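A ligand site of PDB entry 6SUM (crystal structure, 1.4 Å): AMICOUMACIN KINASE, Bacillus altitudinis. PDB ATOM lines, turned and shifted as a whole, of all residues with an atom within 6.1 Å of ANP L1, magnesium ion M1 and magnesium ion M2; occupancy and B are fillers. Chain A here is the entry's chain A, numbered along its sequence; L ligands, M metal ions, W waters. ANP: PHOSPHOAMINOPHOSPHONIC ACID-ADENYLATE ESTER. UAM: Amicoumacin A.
The side-chain amino group (NZ) of Lys 53 lies within salt-bridge range of an oxygen (O1A) of ANP L1 (2.8 Å).
O2' of ANP L1 lies within hydrogen-bond range of NZ of Lys 117 (2.7 Å).
A ring nitrogen (NE2) of His 205 lies close to an oxygen (O1G) of ANP L1, 2.9 Å away.
OD2 of Asp 203 lies within salt-bridge range of NAD of UAM L2 (3.6 Å).
An oxygen (O1B) of ANP L1 lies within hydrogen-bond range of the backbone NH of Asn 37, at 3.0 Å.
OD2 of Asp 223 lies within salt-bridge range of NAD of UAM L2, at 2.8 Å.
O3' of ANP L1 lies within hydrogen-bond range of O of Gly 207.
N of Gly 207 sits at hydrogen-bond distance from OAH of UAM L2.
O1B of ANP L1 lies within hydrogen-bond range of N of Glu 36, 3.1 Å away.
The side-chain amide nitrogen (ND2) of Asn 37 lies within hydrogen-bond range of an oxygen (O1B) of ANP L1 (3.5 Å).
The backbone NH (N) of Ala 113 sits at hydrogen-bond distance from a nitrogen (N1) of ANP L1, at 2.9 Å.
A nitrogen (N6) of ANP L1 is in hydrogen-bond range of the backbone carbonyl oxygen of Glu 111, at 3.0 Å.
The side-chain carboxylate of Glu 36 is in salt-bridge range of a nitrogen (NAD) of UAM L2 (3.1 Å).
An oxygen (O3G) of ANP L1 lies within hydrogen-bond range of an oxygen (OAI) of UAM L2, at 3.2 Å.
The backbone NH (N) of Phe 219 sits at hydrogen-bond distance from the backbone carbonyl oxygen (O) of Asn 208.
The backbone carbonyl oxygen (O) of Val 39 is in hydrogen-bond range of the backbone NH (N) of Leu 32, 2.8 Å away.
ND2 of Asn 208 is in hydrogen-bond range of NE2 of His 205, at 3.1 Å.
O of Ile 51 sits at hydrogen-bond distance from N of Tyr 110.
The backbone carbonyl oxygen of Pro 114 sits at hydrogen-bond distance from a ring nitrogen (ND1) of His 210 (3.0 Å).
N of Gly 207 sits at hydrogen-bond distance from ND1 of His 205, at 2.9 Å.
A ring nitrogen (ND1) of His 210 sits at hydrogen-bond distance from the backbone carbonyl oxygen of Ala 113, at 3.1 Å.
NZ of Lys 53 lies close to OD1 of Asp 220 (3.1 Å).
Merely in contact with ANP L1: Ala 83, Phe 219, Ala 35, Lys 112, Asp 203, Val 39, His 210, Ile 51 and Leu 32.
Hydrophobic or aromatic side chains that line ANP L1: Leu 32, Ala 35, Val 39, Ile 51, Ala 83, Ala 113, His 205, His 210 and Phe 219.
19 residues have an atom within 4 Å of ANP L1: Leu 32, Ala 35, Glu 36, Asn 37, Val 39, Ile 51, Lys 53, Ala 83, Glu 111, Lys 112, Ala 113, Lys 117, Asp 203, His 205, Gly 207, Asn 208, His 210, Phe 219 and Asp 220.
The nearest printed residue that does not touch ANP L1 is Ala 33 (4.2 Å).
Residues that only touch magnesium ion M1: Asp 223 (3.8 Å).
Within 4 Å of magnesium ion M1: Asp 220 and Asp 223.
Residues that only touch magnesium ion M2: His 205 (3.8 Å).
Three residues have an atom within 4 Å of magnesium ion M2: His 205, Asn 208 and Asp 220.
Along chain A the residues within 4 Å of magnesium ion M2 span positions 205 to 220.
The nearest printed residue that does not touch magnesium ion M2 is Gly 207 (4.3 Å).
An oxygen (O2G) of ANP L1 is bound to magnesium ion M1, at 2.0 Å.
O2B of ANP L1 is bound to magnesium ion M1 (2.0 Å).
Water W5 is bound to magnesium ion M1, at 2.1 Å.
Magnesium ion M1 is bound by water W7.
Magnesium ion M1 is bound by OD2 of Asp 220, 2.1 Å away.
Magnesium ion M1 is bound by OD1 of Asp 220, 2.2 Å away.
Magnesium ion M2 is bound by O2A of ANP L1 (1.9 Å), O1G of ANP L1 (1.9 Å), OD1 of Asn 208 (2.0 Å), OD2 of Asp 220 (2.1 Å) and water W4 (2.3 Å).
Magnesium ion M2 has five donor atoms within binding distance.
Slightly farther from magnesium ion M2 lies a nitrogen (N3B) of ANP L1 (2.7 Å).
Water W5 lies within hydrogen-bond range of the side-chain carboxylate (OD2) of Asp 223 (2.7 Å) and the side-chain carboxylate (OD2) of Asp 222 (2.8 Å).
Water W7 lies within hydrogen-bond range of OD2 of Asp 203 (2.7 Å) and OD2 of Asp 223 (2.7 Å).
Water W13 lies within hydrogen-bond range of an oxygen (O3G) of ANP L1 (2.7 Å) and an oxygen (OAG) of UAM L2 (2.9 Å).
Water W8 lies within hydrogen-bond range of O1A of ANP L1 (2.7 Å) and N of Asp 220 (2.9 Å).
Water W1 lies within hydrogen-bond range of a ring nitrogen (NE2) of His 210 and an oxygen (O2') of ANP L1.
Water W2 lies within hydrogen-bond range of an oxygen (OAG) of UAM L2 and an oxygen (O3') of ANP L1.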
ATOM      1  N   LEU A  32      -9.926  18.712  23.724  1.00  0.00           N
ATOM      2  CA  LEU A  32      -9.052  19.890  23.836  1.00  0.00           C
ATOM      3  C   LEU A  32      -9.618  20.953  24.763  1.00  0.00           C
ATOM      4  O   LEU A  32      -8.903  21.396  25.671  1.00  0.00           O
ATOM      5  CB  LEU A  32      -8.755  20.484  22.464  1.00  0.00           C
ATOM      6  CG  LEU A  32      -8.045  19.551  21.475  1.00  0.00           C
ATOM      7  CD1 LEU A  32      -7.783  20.253  20.152  1.00  0.00           C
ATOM      8  CD2 LEU A  32      -6.769  18.960  22.050  1.00  0.00           C
ATOM      9  N   ALA A  33     -10.864  21.378  24.551  1.00  0.00           N
ATOM     10  CA  ALA A  33     -11.451  22.465  25.361  1.00  0.00           C
ATOM     11  C   ALA A  33     -12.956  22.533  25.171  1.00  0.00           C
ATOM     12  O   ALA A  33     -13.499  22.038  24.189  1.00  0.00           O
ATOM     13  CB  ALA A  33     -10.818  23.814  24.978  1.00  0.00           C
ATOM     14  N   ASP A  34     -13.629  23.157  26.127  1.00  0.00           N
ATOM     15  CA  ASP A  34     -15.059  23.348  26.093  1.00  0.00           C
ATOM     16  C   ASP A  34     -15.445  24.745  26.557  1.00  0.00           C
ATOM     17  O   ASP A  34     -16.293  24.920  27.453  1.00  0.00           O
ATOM     18  CB  ASP A  34     -15.800  22.280  26.901  1.00  0.00           C
ATOM     19  CG  ASP A  34     -15.464  22.283  28.407  1.00  0.00           C
ATOM     20  OD1 ASP A  34     -14.496  22.929  28.850  1.00  0.00           O
ATOM     21  OD2 ASP A  34     -16.206  21.616  29.150  1.00  0.00           O
ATOM     22  N   ALA A  35     -14.807  25.736  25.943  1.00  0.00           N
ATOM     23  CA  ALA A  35     -15.080  27.129  26.237  1.00  0.00           C
ATOM     24  C   ALA A  35     -16.395  27.520  25.550  1.00  0.00           C
ATOM     25  O   ALA A  35     -17.429  27.388  26.157  1.00  0.00           O
ATOM     26  CB  ALA A  35     -13.916  28.008  25.827  1.00  0.00           C
ATOM     27  N   GLU A  36     -16.383  27.907  24.289  1.00  0.00           N
ATOM     28  CA  GLU A  36     -17.602  28.286  23.541  1.00  0.00           C
ATOM     29  C   GLU A  36     -18.171  27.094  22.750  1.00  0.00           C
ATOM     30  O   GLU A  36     -19.359  27.016  22.509  1.00  0.00           O
ATOM     31  CB  GLU A  36     -17.245  29.388  22.541  1.00  0.00           C
ATOM     32  CG  GLU A  36     -18.296  30.446  22.230  1.00  0.00           C
ATOM     33  CD  GLU A  36     -18.480  31.483  23.359  1.00  0.00           C
ATOM     34  OE1 GLU A  36     -18.925  31.067  24.452  1.00  0.00           O
ATOM     35  OE2 GLU A  36     -18.235  32.693  23.158  1.00  0.00           O
ATOM     36  N   ASN A  37     -17.277  26.223  22.291  1.00  0.00           N
ATOM     37  CA  ASN A  37     -17.540  25.029  21.510  1.00  0.00           C
ATOM     38  C   ASN A  37     -16.863  23.859  22.205  1.00  0.00           C
ATOM     39  O   ASN A  37     -15.916  24.046  22.975  1.00  0.00           O
ATOM     40  CB  ASN A  37     -16.879  25.179  20.151  1.00  0.00           C
ATOM     41  CG  ASN A  37     -17.471  26.318  19.337  1.00  0.00           C
ATOM     42  OD1 ASN A  37     -18.448  26.121  18.642  1.00  0.00           O
ATOM     43  ND2 ASN A  37     -16.859  27.494  19.413  1.00  0.00           N
ATOM     44  N   TYR A  38     -17.321  22.638  21.898  1.00  0.00           N
ATOM     45  CA  TYR A  38     -16.621  21.449  22.347  1.00  0.00           C
ATOM     46  C   TYR A  38     -15.619  21.097  21.245  1.00  0.00           C
ATOM     47  O   TYR A  38     -16.026  20.881  20.099  1.00  0.00           O
ATOM     48  CB  TYR A  38     -17.598  20.279  22.561  1.00  0.00           C
ATOM     49  CG  TYR A  38     -18.583  20.485  23.649  1.00  0.00           C
ATOM     50  CD1 TYR A  38     -18.241  20.283  24.997  1.00  0.00           C
ATOM     51  CD2 TYR A  38     -19.884  20.910  23.359  1.00  0.00           C
ATOM     52  CE1 TYR A  38     -19.180  20.468  26.017  1.00  0.00           C
ATOM     53  CE2 TYR A  38     -20.802  21.109  24.362  1.00  0.00           C
ATOM     54  CZ  TYR A  38     -20.464  20.886  25.682  1.00  0.00           C
ATOM     55  OH  TYR A  38     -21.431  21.090  26.632  1.00  0.00           O
ATOM     56  N   VAL A  39     -14.322  21.067  21.578  1.00  0.00           N
ATOM     57  CA  VAL A  39     -13.278  20.952  20.572  1.00  0.00           C
ATOM     58  C   VAL A  39     -12.415  19.738  20.898  1.00  0.00           C
ATOM     59  O   VAL A  39     -11.995  19.524  22.053  1.00  0.00           O
ATOM     60  CB  VAL A  39     -12.426  22.246  20.490  1.00  0.00           C
ATOM     61  CG1 VAL A  39     -11.369  22.164  19.391  1.00  0.00           C
ATOM     62  CG2 VAL A  39     -13.326  23.462  20.237  1.00  0.00           C
ATOM     63  N   ILE A  51      -9.084  18.737  13.581  1.00  0.00           N
ATOM     64  CA  ILE A  51      -9.721  19.439  14.686  1.00  0.00           C
ATOM     65  C   ILE A  51     -11.229  19.431  14.428  1.00  0.00           C
ATOM     66  O   ILE A  51     -11.677  19.981  13.411  1.00  0.00           O
ATOM     67  CB  ILE A  51      -9.200  20.894  14.846  1.00  0.00           C
ATOM     68  CG1 ILE A  51      -7.679  20.920  15.092  1.00  0.00           C
ATOM     69  CG2 ILE A  51     -10.009  21.617  15.917  1.00  0.00           C
ATOM     70  CD1 ILE A  51      -7.173  20.129  16.284  1.00  0.00           C
ATOM     71  N   LYS A  53     -14.898  20.676  15.838  1.00  0.00           N
ATOM     72  CA  LYS A  53     -15.574  21.663  16.677  1.00  0.00           C
ATOM     73  C   LYS A  53     -17.079  21.324  16.663  1.00  0.00           C
ATOM     74  O   LYS A  53     -17.675  21.190  15.568  1.00  0.00           O
ATOM     75  CB  LYS A  53     -15.302  23.044  16.097  1.00  0.00           C
ATOM     76  CG  LYS A  53     -16.030  24.146  16.811  1.00  0.00           C
ATOM     77  CD  LYS A  53     -15.557  25.525  16.405  1.00  0.00           C
ATOM     78  CE  LYS A  53     -14.275  25.920  17.093  1.00  0.00           C
ATOM     79  NZ  LYS A  53     -14.015  27.403  17.037  1.00  0.00           N
ATOM     80  N   ALA A  83      -6.249  28.317   9.315  1.00  0.00           N
ATOM     81  CA  ALA A  83      -6.601  26.904   9.310  1.00  0.00           C
ATOM     82  C   ALA A  83      -7.870  26.680   8.480  1.00  0.00           C
ATOM     83  O   ALA A  83      -8.934  27.200   8.790  1.00  0.00           O
ATOM     84  CB  ALA A  83      -6.770  26.371  10.713  1.00  0.00           C
ATOM     85  N   TYR A 110     -11.576  21.146  10.831  1.00  0.00           N
ATOM     86  CA  TYR A 110     -10.545  21.980  10.262  1.00  0.00           C
ATOM     87  C   TYR A 110      -9.213  21.230  10.229  1.00  0.00           C
ATOM     88  O   TYR A 110      -8.961  20.332  11.022  1.00  0.00           O
ATOM     89  CB  TYR A 110     -10.355  23.238  11.103  1.00  0.00           C
ATOM     90  CG  TYR A 110     -11.558  24.133  11.281  1.00  0.00           C
ATOM     91  CD1 TYR A 110     -12.461  23.886  12.288  1.00  0.00           C
ATOM     92  CD2 TYR A 110     -11.761  25.242  10.462  1.00  0.00           C
ATOM     93  CE1 TYR A 110     -13.523  24.720  12.517  1.00  0.00           C
ATOM     94  CE2 TYR A 110     -12.858  26.076  10.662  1.00  0.00           C
ATOM     95  CZ  TYR A 110     -13.737  25.795  11.704  1.00  0.00           C
ATOM     96  OH  TYR A 110     -14.812  26.605  11.986  1.00  0.00           O
ATOM     97  N   GLU A 111      -8.349  21.673   9.339  1.00  0.00           N
ATOM     98  CA  GLU A 111      -6.946  21.286   9.364  1.00  0.00           C
ATOM     99  C   GLU A 111      -6.294  21.751  10.663  1.00  0.00           C
ATOM    100  O   GLU A 111      -6.594  22.834  11.164  1.00  0.00           O
ATOM    101  CB  GLU A 111      -6.199  21.831   8.139  1.00  0.00           C
ATOM    102  CG  GLU A 111      -6.744  21.242   6.829  1.00  0.00           C
ATOM    103  CD  GLU A 111      -5.953  21.536   5.564  1.00  0.00           C
ATOM    104  OE1 GLU A 111      -5.187  22.513   5.504  1.00  0.00           O
ATOM    105  OE2 GLU A 111      -6.117  20.768   4.587  1.00  0.00           O
ATOM    106  N   LYS A 112      -5.465  20.901  11.247  1.00  0.00           N
ATOM    107  CA  LYS A 112      -4.657  21.282  12.395  1.00  0.00           C
ATOM    108  C   LYS A 112      -3.531  22.192  11.948  1.00  0.00           C
ATOM    109  O   LYS A 112      -2.696  21.807  11.125  1.00  0.00           O
ATOM    110  CB  LYS A 112      -4.124  20.052  13.128  1.00  0.00           C
ATOM    111  CG  LYS A 112      -3.373  20.405  14.415  1.00  0.00           C
ATOM    112  CD  LYS A 112      -3.043  19.180  15.263  1.00  0.00           C
ATOM    113  CE  LYS A 112      -2.469  19.633  16.605  1.00  0.00           C
ATOM    114  NZ  LYS A 112      -1.807  18.563  17.403  1.00  0.00           N
ATOM    115  N   ALA A 113      -3.505  23.403  12.480  1.00  0.00           N
ATOM    116  CA  ALA A 113      -2.465  24.359  12.139  1.00  0.00           C
ATOM    117  C   ALA A 113      -1.110  23.841  12.616  1.00  0.00           C
ATOM    118  O   ALA A 113      -0.995  23.375  13.756  1.00  0.00           O
ATOM    119  CB  ALA A 113      -2.743  25.703  12.786  1.00  0.00           C
ATOM    120  N   PRO A 114      -0.069  23.976  11.760  1.00  0.00           N
ATOM    121  CA  PRO A 114       1.269  23.612  12.229  1.00  0.00           C
ATOM    122  C   PRO A 114       1.804  24.613  13.253  1.00  0.00           C
ATOM    123  O   PRO A 114       1.113  25.603  13.577  1.00  0.00           O
ATOM    124  CB  PRO A 114       2.112  23.645  10.941  1.00  0.00           C
ATOM    125  CG  PRO A 114       1.405  24.571  10.024  1.00  0.00           C
ATOM    126  CD  PRO A 114      -0.062  24.434  10.359  1.00  0.00           C
ATOM    127  N   LYS A 117       1.426  27.193  20.037  1.00  0.00           N
ATOM    128  CA  LYS A 117       1.098  28.397  20.789  1.00  0.00           C
ATOM    129  C   LYS A 117       2.365  29.190  21.140  1.00  0.00           C
ATOM    130  O   LYS A 117       3.422  28.608  21.367  1.00  0.00           O
ATOM    131  CB  LYS A 117       0.377  28.042  22.098  1.00  0.00           C
ATOM    132  CG  LYS A 117      -0.915  27.231  21.943  1.00  0.00           C
ATOM    133  CD  LYS A 117      -1.994  28.090  21.369  1.00  0.00           C
ATOM    134  CE  LYS A 117      -3.359  27.419  21.244  1.00  0.00           C
ATOM    135  NZ  LYS A 117      -4.035  26.935  22.475  1.00  0.00           N
ATOM    136  N   ASP A 203     -12.031  38.004  17.556  1.00  0.00           N
ATOM    137  CA  ASP A 203     -11.591  37.351  18.789  1.00  0.00           C
ATOM    138  C   ASP A 203     -10.111  36.999  18.736  1.00  0.00           C
ATOM    139  O   ASP A 203      -9.696  35.895  19.082  1.00  0.00           O
ATOM    140  CB  ASP A 203     -12.429  36.122  19.141  1.00  0.00           C
ATOM    141  CG  ASP A 203     -12.192  35.643  20.550  1.00  0.00           C
ATOM    142  OD1 ASP A 203     -11.871  36.488  21.427  1.00  0.00           O
ATOM    143  OD2 ASP A 203     -12.296  34.425  20.825  1.00  0.00           O
ATOM    144  N   HIS A 205      -6.635  36.449  19.912  1.00  0.00           N
ATOM    145  CA  HIS A 205      -5.906  36.194  21.140  1.00  0.00           C
ATOM    146  C   HIS A 205      -4.974  35.008  20.890  1.00  0.00           C
ATOM    147  O   HIS A 205      -5.145  34.304  19.900  1.00  0.00           O
ATOM    148  CB  HIS A 205      -6.803  35.961  22.366  1.00  0.00           C
ATOM    149  CG  HIS A 205      -7.706  34.773  22.328  1.00  0.00           C
ATOM    150  ND1 HIS A 205      -7.241  33.476  22.425  1.00  0.00           N
ATOM    151  CD2 HIS A 205      -9.058  34.684  22.412  1.00  0.00           C
ATOM    152  CE1 HIS A 205      -8.258  32.647  22.464  1.00  0.00           C
ATOM    153  NE2 HIS A 205      -9.378  33.350  22.475  1.00  0.00           N
ATOM    154  N   GLY A 207      -4.636  32.132  22.291  1.00  0.00           N
ATOM    155  CA  GLY A 207      -5.228  30.800  22.156  1.00  0.00           C
ATOM    156  C   GLY A 207      -5.805  30.502  20.787  1.00  0.00           C
ATOM    157  O   GLY A 207      -6.195  29.359  20.527  1.00  0.00           O
ATOM    158  N   ASN A 208      -5.832  31.518  19.906  1.00  0.00           N
ATOM    159  CA  ASN A 208      -6.478  31.435  18.600  1.00  0.00           C
ATOM    160  C   ASN A 208      -5.547  31.546  17.406  1.00  0.00           C
ATOM    161  O   ASN A 208      -5.996  31.757  16.285  1.00  0.00           O
ATOM    162  CB  ASN A 208      -7.593  32.499  18.488  1.00  0.00           C
ATOM    163  CG  ASN A 208      -8.820  32.144  19.291  1.00  0.00           C
ATOM    164  OD1 ASN A 208      -8.962  31.014  19.824  1.00  0.00           O
ATOM    165  ND2 ASN A 208      -9.718  33.123  19.442  1.00  0.00           N
ATOM    166  N   HIS A 210      -1.410  29.942  15.976  1.00  0.00           N
ATOM    167  CA  HIS A 210      -0.110  29.285  16.189  1.00  0.00           C
ATOM    168  C   HIS A 210       0.962  30.148  15.586  1.00  0.00           C
ATOM    169  O   HIS A 210       0.740  30.886  14.640  1.00  0.00           O
ATOM    170  CB  HIS A 210      -0.072  27.922  15.530  1.00  0.00           C
ATOM    171  CG  HIS A 210      -0.692  26.856  16.359  1.00  0.00           C
ATOM    172  ND1 HIS A 210      -0.767  25.543  15.932  1.00  0.00           N
ATOM    173  CD2 HIS A 210      -1.270  26.884  17.578  1.00  0.00           C
ATOM    174  CE1 HIS A 210      -1.365  24.823  16.853  1.00  0.00           C
ATOM    175  NE2 HIS A 210      -1.681  25.607  17.862  1.00  0.00           N
ATOM    176  N   PHE A 219      -6.846  30.713  13.664  1.00  0.00           N
ATOM    177  CA  PHE A 219      -8.015  29.857  13.635  1.00  0.00           C
ATOM    178  C   PHE A 219      -9.077  30.457  14.574  1.00  0.00           C
ATOM    179  O   PHE A 219      -8.965  31.630  14.993  1.00  0.00           O
ATOM    180  CB  PHE A 219      -7.648  28.372  13.947  1.00  0.00           C
ATOM    181  CG  PHE A 219      -6.734  28.191  15.115  1.00  0.00           C
ATOM    182  CD1 PHE A 219      -5.379  27.977  14.893  1.00  0.00           C
ATOM    183  CD2 PHE A 219      -7.194  28.231  16.435  1.00  0.00           C
ATOM    184  CE1 PHE A 219      -4.499  27.809  15.951  1.00  0.00           C
ATOM    185  CE2 PHE A 219      -6.299  28.056  17.499  1.00  0.00           C
ATOM    186  CZ  PHE A 219      -4.965  27.844  17.248  1.00  0.00           C
ATOM    187  N   ASP A 220     -10.118  29.710  14.893  1.00  0.00           N
ATOM    188  CA  ASP A 220     -11.233  30.178  15.712  1.00  0.00           C
ATOM    189  C   ASP A 220     -11.822  31.479  15.166  1.00  0.00           C
ATOM    190  O   ASP A 220     -11.891  32.486  15.872  1.00  0.00           O
ATOM    191  CB  ASP A 220     -10.867  30.298  17.188  1.00  0.00           C
ATOM    192  CG  ASP A 220     -12.077  30.462  18.079  1.00  0.00           C
ATOM    193  OD1 ASP A 220     -13.263  30.358  17.619  1.00  0.00           O
ATOM    194  OD2 ASP A 220     -11.878  30.669  19.323  1.00  0.00           O
ATOM    195  N   PHE A 221     -12.287  31.419  13.918  1.00  0.00           N
ATOM    196  CA  PHE A 221     -13.026  32.500  13.280  1.00  0.00           C
ATOM    197  C   PHE A 221     -14.531  32.448  13.618  1.00  0.00           C
ATOM    198  O   PHE A 221     -15.333  33.140  12.985  1.00  0.00           O
ATOM    199  CB  PHE A 221     -12.841  32.432  11.755  1.00  0.00           C
ATOM    200  CG  PHE A 221     -11.480  32.907  11.266  1.00  0.00           C
ATOM    201  CD1 PHE A 221     -10.344  32.097  11.379  1.00  0.00           C
ATOM    202  CD2 PHE A 221     -11.329  34.165  10.685  1.00  0.00           C
ATOM    203  CE1 PHE A 221      -9.105  32.565  10.961  1.00  0.00           C
ATOM    204  CE2 PHE A 221     -10.102  34.622  10.256  1.00  0.00           C
ATOM    205  CZ  PHE A 221      -8.994  33.800  10.357  1.00  0.00           C
ATOM    206  N   ASP A 222     -14.905  31.677  14.627  1.00  0.00           N
ATOM    207  CA  ASP A 222     -16.301  31.408  14.979  1.00  0.00           C
ATOM    208  C   ASP A 222     -17.092  32.643  15.358  1.00  0.00           C
ATOM    209  O   ASP A 222     -18.312  32.618  15.277  1.00  0.00           O
ATOM    210  CB  ASP A 222     -16.320  30.368  16.119  1.00  0.00           C
ATOM    211  CG  ASP A 222     -17.696  29.960  16.566  1.00  0.00           C
ATOM    212  OD1 ASP A 222     -18.557  29.666  15.692  1.00  0.00           O
ATOM    213  OD2 ASP A 222     -17.868  29.866  17.805  1.00  0.00           O
ATOM    214  N   ASP A 223     -16.413  33.700  15.802  1.00  0.00           N
ATOM    215  CA  ASP A 223     -17.086  34.959  16.168  1.00  0.00           C
ATOM    216  C   ASP A 223     -16.907  36.070  15.152  1.00  0.00           C
ATOM    217  O   ASP A 223     -17.272  37.218  15.413  1.00  0.00           O
ATOM    218  CB  ASP A 223     -16.682  35.395  17.575  1.00  0.00           C
ATOM    219  CG  ASP A 223     -17.192  34.436  18.601  1.00  0.00           C
ATOM    220  OD1 ASP A 223     -18.437  34.277  18.695  1.00  0.00           O
ATOM    221  OD2 ASP A 223     -16.355  33.799  19.286  1.00  0.00           O
HETATM  222  PG  ANP L   1     -12.684  30.679  22.477  1.00  0.00           P
HETATM  223  O1G ANP L   1     -11.272  31.188  22.109  1.00  0.00           O
HETATM  224  O2G ANP L   1     -13.788  31.263  21.635  1.00  0.00           O
HETATM  225  O3G ANP L   1     -12.875  30.812  23.988  1.00  0.00           O
HETATM  226  PB  ANP L   1     -13.568  28.063  21.156  1.00  0.00           P
HETATM  227  O1B ANP L   1     -14.517  27.209  21.942  1.00  0.00           O
HETATM  228  O2B ANP L   1     -14.132  28.895  20.078  1.00  0.00           O
HETATM  229  N3B ANP L   1     -12.584  28.998  22.155  1.00  0.00           N
HETATM  230  PA  ANP L   1     -11.181  27.151  19.650  1.00  0.00           P
HETATM  231  O1A ANP L   1     -11.521  27.174  18.195  1.00  0.00           O
HETATM  232  O2A ANP L   1     -10.315  28.236  20.191  1.00  0.00           O
HETATM  233  O3A ANP L   1     -12.506  27.010  20.550  1.00  0.00           O
HETATM  234  O5' ANP L   1     -10.500  25.731  19.941  1.00  0.00           O
HETATM  235  C5' ANP L   1      -9.988  25.370  21.205  1.00  0.00           C
HETATM  236  C4' ANP L   1      -8.503  25.085  21.173  1.00  0.00           C
HETATM  237  O4' ANP L   1      -8.277  24.016  20.230  1.00  0.00           O
HETATM  238  C3' ANP L   1      -7.607  26.211  20.692  1.00  0.00           C
HETATM  239  O3' ANP L   1      -7.262  27.132  21.718  1.00  0.00           O
HETATM  240  C2' ANP L   1      -6.409  25.447  20.170  1.00  0.00           C
HETATM  241  O2' ANP L   1      -5.557  25.021  21.238  1.00  0.00           O
HETATM  242  C1' ANP L   1      -7.060  24.245  19.528  1.00  0.00           C
HETATM  243  N9  ANP L   1      -7.380  24.459  18.110  1.00  0.00           N
HETATM  244  C8  ANP L   1      -8.551  24.919  17.599  1.00  0.00           C
HETATM  245  N7  ANP L   1      -8.508  24.992  16.264  1.00  0.00           N
HETATM  246  C5  ANP L   1      -7.266  24.602  15.921  1.00  0.00           C
HETATM  247  C6  ANP L   1      -6.583  24.404  14.663  1.00  0.00           C
HETATM  248  N6  ANP L   1      -7.212  24.639  13.513  1.00  0.00           N
HETATM  249  N1  ANP L   1      -5.300  23.946  14.692  1.00  0.00           N
HETATM  250  C2  ANP L   1      -4.696  23.675  15.865  1.00  0.00           C
HETATM  251  N3  ANP L   1      -5.284  23.801  17.064  1.00  0.00           N
HETATM  252  C4  ANP L   1      -6.547  24.259  17.116  1.00  0.00           C
HETATM  253  CAO UAM L   2      -9.602  34.847  26.275  1.00  0.00           C
HETATM  254  CAW UAM L   2      -8.111  34.620  26.069  1.00  0.00           C
HETATM  255  CAM UAM L   2      -7.215  35.688  26.097  1.00  0.00           C
HETATM  256  CAK UAM L   2      -5.856  35.434  25.888  1.00  0.00           C
HETATM  257  CAL UAM L   2      -5.396  34.129  25.673  1.00  0.00           C
HETATM  258  CAV UAM L   2      -6.302  33.089  25.649  1.00  0.00           C
HETATM  259  OAH UAM L   2      -5.875  31.829  25.415  1.00  0.00           O
HETATM  260  CAX UAM L   2      -7.645  33.328  25.854  1.00  0.00           C
HETATM  261  CAU UAM L   2      -8.627  32.214  25.806  1.00  0.00           C
HETATM  262  OAG UAM L   2      -8.406  31.112  25.407  1.00  0.00           O
HETATM  263  OAR UAM L   2      -9.951  32.430  26.179  1.00  0.00           O
HETATM  264  CBD UAM L   2     -10.214  33.622  26.939  1.00  0.00           C
HETATM  265  CBC UAM L   2     -11.722  33.709  27.061  1.00  0.00           C
HETATM  266  CAP UAM L   2     -12.289  32.465  27.745  1.00  0.00           C
HETATM  267  CAY UAM L   2     -13.773  32.535  28.075  1.00  0.00           C
HETATM  268  CAB UAM L   2     -14.105  31.266  28.847  1.00  0.00           C
HETATM  269  CAA UAM L   2     -14.196  33.750  28.871  1.00  0.00           C
HETATM  270  NAQ UAM L   2     -12.331  33.880  25.722  1.00  0.00           N
HETATM  271  CAT UAM L   2     -12.864  35.028  25.332  1.00  0.00           C
HETATM  272  OAF UAM L   2     -12.944  36.001  26.044  1.00  0.00           O
HETATM  273  CBA UAM L   2     -13.419  35.105  23.927  1.00  0.00           C
HETATM  274  OAI UAM L   2     -13.140  33.891  23.220  1.00  0.00           O
HETATM  275  CBB UAM L   2     -14.930  35.309  23.954  1.00  0.00           C
HETATM  276  OAJ UAM L   2     -15.177  36.562  24.627  1.00  0.00           O
HETATM  277  CAZ UAM L   2     -15.536  35.393  22.565  1.00  0.00           C
HETATM  278  NAD UAM L   2     -15.664  34.018  22.011  1.00  0.00           N
HETATM  279  CAN UAM L   2     -16.913  36.025  22.663  1.00  0.00           C
HETATM  280  CAS UAM L   2     -17.428  36.486  21.333  1.00  0.00           C
HETATM  281  OAE UAM L   2     -16.676  36.731  20.408  1.00  0.00           O
HETATM  282  NAC UAM L   2     -18.728  36.666  21.251  1.00  0.00           N
HETATM  283 MG    MG M   1     -13.983  30.879  19.685  1.00  0.00          MG
HETATM  284 MG    MG M   2     -10.479  30.046  20.746  1.00  0.00          MG
HETATM  285  O   HOH W   1      -3.030  24.558  19.796  1.00  0.00           O
HETATM  286  O   HOH W   2      -6.771  28.729  24.740  1.00  0.00           O
HETATM  287  O   HOH W   3     -13.336  25.294  23.436  1.00  0.00           O
HETATM  288  O   HOH W   4      -9.183  29.309  22.497  1.00  0.00           O
HETATM  289  O   HOH W   5     -16.020  31.132  19.423  1.00  0.00           O
HETATM  290  O   HOH W   6      -8.367  26.393  24.843  1.00  0.00           O
HETATM  291  O   HOH W   7     -13.789  32.920  19.194  1.00  0.00           O
HETATM  292  O   HOH W   8     -10.496  26.903  15.671  1.00  0.00           O
HETATM  293  O   HOH W   9      -9.953  25.915  13.153  1.00  0.00           O
HETATM  294  O   HOH W  10     -11.017  27.110  24.006  1.00  0.00           O
HETATM  295  O   HOH W  11      -3.837  22.219  18.906  1.00  0.00           O
HETATM  296  O   HOH W  12     -15.156  31.744  25.156  1.00  0.00           O
HETATM  297  O   HOH W  13     -10.856  29.641  25.318  1.00  0.00           O
HETATM  298  O   HOH W  14      -5.723  22.798  22.773  1.00  0.00           O
